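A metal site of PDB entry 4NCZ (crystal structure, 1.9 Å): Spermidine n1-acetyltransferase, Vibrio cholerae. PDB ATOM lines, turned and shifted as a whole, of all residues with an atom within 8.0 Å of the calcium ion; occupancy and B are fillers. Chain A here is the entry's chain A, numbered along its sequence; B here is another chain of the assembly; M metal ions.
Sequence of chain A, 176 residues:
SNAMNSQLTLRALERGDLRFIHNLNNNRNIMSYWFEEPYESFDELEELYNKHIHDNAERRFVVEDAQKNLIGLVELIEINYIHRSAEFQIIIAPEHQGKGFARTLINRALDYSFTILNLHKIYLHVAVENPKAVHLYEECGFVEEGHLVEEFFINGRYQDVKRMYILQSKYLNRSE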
ATOM      1  N   PHE A  35      -6.060  11.187 -36.910  1.00  0.00           N
ATOM      2  CA  PHE A  35      -6.091  10.976 -35.450  1.00  0.00           C
ATOM      3  C   PHE A  35      -4.901  11.663 -34.805  1.00  0.00           C
ATOM      4  O   PHE A  35      -4.195  11.074 -33.974  1.00  0.00           O
ATOM      5  CB  PHE A  35      -6.155   9.489 -35.127  1.00  0.00           C
ATOM      6  CG  PHE A  35      -7.469   8.903 -35.436  1.00  0.00           C
ATOM      7  CD1 PHE A  35      -7.800   8.532 -36.730  1.00  0.00           C
ATOM      8  CD2 PHE A  35      -8.412   8.744 -34.425  1.00  0.00           C
ATOM      9  CE1 PHE A  35      -9.050   8.018 -37.021  1.00  0.00           C
ATOM     10  CE2 PHE A  35      -9.663   8.254 -34.688  1.00  0.00           C
ATOM     11  CZ  PHE A  35      -9.989   7.891 -35.984  1.00  0.00           C
ATOM     12  N   GLU A  36      -4.649  12.908 -35.235  1.00  0.00           N
ATOM     13  CA  GLU A  36      -3.563  13.785 -34.724  1.00  0.00           C
ATOM     14  C   GLU A  36      -2.137  13.309 -35.001  1.00  0.00           C
ATOM     15  O   GLU A  36      -1.216  13.834 -34.430  1.00  0.00           O
ATOM     16  CB  GLU A  36      -3.795  14.103 -33.212  1.00  0.00           C
ATOM     17  CG  GLU A  36      -5.222  14.505 -32.966  1.00  0.00           C
ATOM     18  CD  GLU A  36      -5.462  14.974 -31.502  1.00  0.00           C
ATOM     19  OE1 GLU A  36      -5.048  16.079 -31.145  1.00  0.00           O
ATOM     20  OE2 GLU A  36      -6.043  14.206 -30.716  1.00  0.00           O
ATOM     21  N   ALA A  57     -12.848   8.762 -31.749  1.00  0.00           N
ATOM     22  CA  ALA A  57     -12.609  10.190 -31.629  1.00  0.00           C
ATOM     23  C   ALA A  57     -12.711  10.936 -32.969  1.00  0.00           C
ATOM     24  O   ALA A  57     -12.812  12.159 -32.994  1.00  0.00           O
ATOM     25  CB  ALA A  57     -11.254  10.426 -31.008  1.00  0.00           C
ATOM     26  N   GLU A  58     -12.713  10.200 -34.087  1.00  0.00           N
ATOM     27  CA  GLU A  58     -12.849  10.840 -35.385  1.00  0.00           C
ATOM     28  C   GLU A  58     -13.711   9.929 -36.222  1.00  0.00           C
ATOM     29  O   GLU A  58     -13.629   8.721 -36.029  1.00  0.00           O
ATOM     30  CB  GLU A  58     -11.500  11.129 -36.060  1.00  0.00           C
ATOM     31  CG  GLU A  58     -10.512  11.924 -35.218  1.00  0.00           C
ATOM     32  CD  GLU A  58      -9.174  12.277 -35.888  1.00  0.00           C
ATOM     33  OE1 GLU A  58      -8.416  13.094 -35.243  1.00  0.00           O
ATOM     34  OE2 GLU A  58      -8.875  11.822 -37.067  1.00  0.00           O
ATOM     35  N   ILE A  77     -13.755  15.440 -36.120  1.00  0.00           N
ATOM     36  CA  ILE A  77     -12.656  15.104 -35.276  1.00  0.00           C
ATOM     37  C   ILE A  77     -12.867  15.735 -33.860  1.00  0.00           C
ATOM     38  O   ILE A  77     -13.822  16.472 -33.639  1.00  0.00           O
ATOM     39  CB  ILE A  77     -11.331  15.541 -35.882  1.00  0.00           C
ATOM     40  CG1 ILE A  77     -11.223  17.062 -35.981  1.00  0.00           C
ATOM     41  CG2 ILE A  77     -11.184  14.978 -37.334  1.00  0.00           C
ATOM     42  CD1 ILE A  77      -9.828  17.528 -36.224  1.00  0.00           C
ATOM     43  N   GLU A  78     -11.946  15.430 -32.958  1.00  0.00           N
ATOM     44  CA  GLU A  78     -11.971  15.845 -31.526  1.00  0.00           C
ATOM     45  C   GLU A  78     -13.329  15.584 -30.914  1.00  0.00           C
ATOM     46  O   GLU A  78     -13.797  16.353 -30.076  1.00  0.00           O
ATOM     47  CB  GLU A  78     -11.603  17.328 -31.402  1.00  0.00           C
ATOM     48  CG  GLU A  78     -10.194  17.718 -31.855  1.00  0.00           C
ATOM     49  CD  GLU A  78      -9.103  17.105 -30.975  1.00  0.00           C
ATOM     50  OE1 GLU A  78      -9.320  17.066 -29.753  1.00  0.00           O
ATOM     51  OE2 GLU A  78      -8.073  16.559 -31.494  1.00  0.00           O
ATOM     52  N   ILE A  79     -13.938  14.453 -31.275  1.00  0.00           N
ATOM     53  CA  ILE A  79     -15.268  14.127 -30.837  1.00  0.00           C
ATOM     54  C   ILE A  79     -15.212  13.828 -29.346  1.00  0.00           C
ATOM     55  O   ILE A  79     -14.389  13.012 -28.885  1.00  0.00           O
ATOM     56  CB  ILE A  79     -15.868  12.938 -31.575  1.00  0.00           C
ATOM     57  CG1 ILE A  79     -15.870  13.207 -33.065  1.00  0.00           C
ATOM     58  CG2 ILE A  79     -17.289  12.719 -31.120  1.00  0.00           C
ATOM     59  CD1 ILE A  79     -16.232  11.982 -33.885  1.00  0.00           C
ATOM     60  N   GLU A  87     -15.281  18.834 -34.033  1.00  0.00           N
ATOM     61  CA  GLU A  87     -14.818  19.800 -35.013  1.00  0.00           C
ATOM     62  C   GLU A  87     -15.083  19.163 -36.382  1.00  0.00           C
ATOM     63  O   GLU A  87     -14.812  18.013 -36.570  1.00  0.00           O
ATOM     64  CB  GLU A  87     -13.346  20.032 -34.820  1.00  0.00           C
ATOM     65  CG  GLU A  87     -12.763  20.990 -35.848  1.00  0.00           C
ATOM     66  CD  GLU A  87     -11.232  21.031 -35.769  1.00  0.00           C
ATOM     67  OE1 GLU A  87     -10.649  20.847 -34.691  1.00  0.00           O
ATOM     68  OE2 GLU A  87     -10.626  21.219 -36.809  1.00  0.00           O
ATOM     69  N   PHE B  35      -4.179  12.349 -21.633  1.00  0.00           N
ATOM     70  CA  PHE B  35      -4.081  12.053 -23.086  1.00  0.00           C
ATOM     71  C   PHE B  35      -5.432  11.726 -23.687  1.00  0.00           C
ATOM     72  O   PHE B  35      -5.581  10.759 -24.484  1.00  0.00           O
ATOM     73  CB  PHE B  35      -3.064  10.938 -23.284  1.00  0.00           C
ATOM     74  CG  PHE B  35      -1.662  11.390 -23.041  1.00  0.00           C
ATOM     75  CD1 PHE B  35      -1.131  11.394 -21.757  1.00  0.00           C
ATOM     76  CD2 PHE B  35      -0.852  11.832 -24.097  1.00  0.00           C
ATOM     77  CE1 PHE B  35       0.145  11.836 -21.495  1.00  0.00           C
ATOM     78  CE2 PHE B  35       0.436  12.299 -23.809  1.00  0.00           C
ATOM     79  CZ  PHE B  35       0.931  12.263 -22.533  1.00  0.00           C
ATOM     80  N   GLU B  36      -6.430  12.561 -23.314  1.00  0.00           N
ATOM     81  CA  GLU B  36      -7.807  12.525 -23.904  1.00  0.00           C
ATOM     82  C   GLU B  36      -8.611  11.288 -23.587  1.00  0.00           C
ATOM     83  O   GLU B  36      -9.665  11.056 -24.164  1.00  0.00           O
ATOM     84  CB  GLU B  36      -7.802  12.869 -25.436  1.00  0.00           C
ATOM     85  CG  GLU B  36      -6.982  14.113 -25.778  1.00  0.00           C
ATOM     86  CD  GLU B  36      -7.011  14.491 -27.285  1.00  0.00           C
ATOM     87  OE1 GLU B  36      -8.079  14.830 -27.785  1.00  0.00           O
ATOM     88  OE2 GLU B  36      -5.954  14.488 -27.961  1.00  0.00           O
ATOM     89  N   ALA B  57       2.639  14.462 -26.731  1.00  0.00           N
ATOM     90  CA  ALA B  57       1.492  15.338 -27.001  1.00  0.00           C
ATOM     91  C   ALA B  57       1.075  16.110 -25.761  1.00  0.00           C
ATOM     92  O   ALA B  57       0.308  17.092 -25.842  1.00  0.00           O
ATOM     93  CB  ALA B  57       0.327  14.538 -27.513  1.00  0.00           C
ATOM     94  N   GLU B  58       1.571  15.676 -24.602  1.00  0.00           N
ATOM     95  CA  GLU B  58       1.248  16.367 -23.332  1.00  0.00           C
ATOM     96  C   GLU B  58       2.460  16.295 -22.454  1.00  0.00           C
ATOM     97  O   GLU B  58       3.199  15.298 -22.499  1.00  0.00           O
ATOM     98  CB  GLU B  58      -0.001  15.780 -22.663  1.00  0.00           C
ATOM     99  CG  GLU B  58      -1.239  15.592 -23.545  1.00  0.00           C
ATOM    100  CD  GLU B  58      -2.522  15.102 -22.870  1.00  0.00           C
ATOM    101  OE1 GLU B  58      -3.610  15.273 -23.531  1.00  0.00           O
ATOM    102  OE2 GLU B  58      -2.499  14.581 -21.705  1.00  0.00           O
ATOM    103  N   ILE B  77      -1.158  20.458 -22.958  1.00  0.00           N
ATOM    104  CA  ILE B  77      -1.722  19.376 -23.728  1.00  0.00           C
ATOM    105  C   ILE B  77      -1.950  19.840 -25.191  1.00  0.00           C
ATOM    106  O   ILE B  77      -1.670  20.967 -25.539  1.00  0.00           O
ATOM    107  CB  ILE B  77      -3.019  18.834 -23.127  1.00  0.00           C
ATOM    108  CG1 ILE B  77      -4.104  19.932 -23.035  1.00  0.00           C
ATOM    109  CG2 ILE B  77      -2.765  18.316 -21.725  1.00  0.00           C
ATOM    110  CD1 ILE B  77      -5.511  19.406 -22.803  1.00  0.00           C
ATOM    111  N   GLU B  78      -2.394  18.920 -26.019  1.00  0.00           N
ATOM    112  CA  GLU B  78      -2.567  19.218 -27.483  1.00  0.00           C
ATOM    113  C   GLU B  78      -1.335  19.839 -28.090  1.00  0.00           C
ATOM    114  O   GLU B  78      -1.433  20.685 -29.010  1.00  0.00           O
ATOM    115  CB  GLU B  78      -3.746  20.166 -27.651  1.00  0.00           C
ATOM    116  CG  GLU B  78      -5.072  19.605 -27.144  1.00  0.00           C
ATOM    117  CD  GLU B  78      -5.645  18.467 -28.029  1.00  0.00           C
ATOM    118  OE1 GLU B  78      -5.430  18.456 -29.245  1.00  0.00           O
ATOM    119  OE2 GLU B  78      -6.272  17.526 -27.490  1.00  0.00           O
ATOM    120  N   ILE B  79      -0.165  19.371 -27.690  1.00  0.00           N
ATOM    121  CA  ILE B  79       1.062  19.954 -28.178  1.00  0.00           C
ATOM    122  C   ILE B  79       1.207  19.531 -29.657  1.00  0.00           C
ATOM    123  O   ILE B  79       1.122  18.370 -29.969  1.00  0.00           O
ATOM    124  CB  ILE B  79       2.284  19.508 -27.400  1.00  0.00           C
ATOM    125  CG1 ILE B  79       2.094  19.799 -25.905  1.00  0.00           C
ATOM    126  CG2 ILE B  79       3.548  20.183 -27.918  1.00  0.00           C
ATOM    127  CD1 ILE B  79       3.244  19.224 -25.135  1.00  0.00           C
ATOM    128  N   GLU B  87      -2.039  23.867 -25.391  1.00  0.00           N
ATOM    129  CA  GLU B  87      -3.041  24.333 -24.496  1.00  0.00           C
ATOM    130  C   GLU B  87      -2.474  24.160 -23.085  1.00  0.00           C
ATOM    131  O   GLU B  87      -1.874  23.174 -22.821  1.00  0.00           O
ATOM    132  CB  GLU B  87      -4.304  23.538 -24.656  1.00  0.00           C
ATOM    133  CG  GLU B  87      -5.383  23.955 -23.614  1.00  0.00           C
ATOM    134  CD  GLU B  87      -6.640  23.097 -23.705  1.00  0.00           C
ATOM    135  OE1 GLU B  87      -6.825  22.411 -24.724  1.00  0.00           O
ATOM    136  OE2 GLU B  87      -7.430  23.095 -22.770  1.00  0.00           O
HETATM  137 CA    CA M   1      -6.920  16.251 -29.436  1.00  0.00          CA
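The backbone NH of Glu 78 of chain A is in hydrogen-bond range of the backbone carbonyl oxygen of Ala 57 of chain A, at 3.4 Å. The backbone carbonyl oxygen of Ala 57 of chain B lies within hydrogen-bond range of the backbone NH of Glu 78 of chain B, at 3.3 Å.
Four residues have an atom within 4 Å of the calcium ion: Glu 36 of chain A, Glu 78 of chain A, Glu 36 of chain B and Glu 78 of chain B. The nearest printed residue that does not touch the calcium ion is Glu 58 of chain A (6.8 Å).
The calcium ion is bound by the side-chain carboxylate (OE2) of Glu 78 of chain A (2.4 Å), the side-chain carboxylate (OE2) of Glu 78 of chain B (2.4 Å), the side-chain carboxylate (OE1) of Glu 36 of chain B (2.5 Å), the side-chain carboxylate (OE2) of Glu 36 of chain B (2.5 Å), the side-chain carboxylate (OE1) of Glu 36 of chain A (2.5 Å), the side-chain carboxylate (OE1) of Glu 78 of chain A (2.6 Å), the side-chain carboxylate (OE2) of Glu 36 of chain A (2.6 Å) and the side-chain carboxylate (OE1) of Glu 78 of chain B (2.7 Å).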
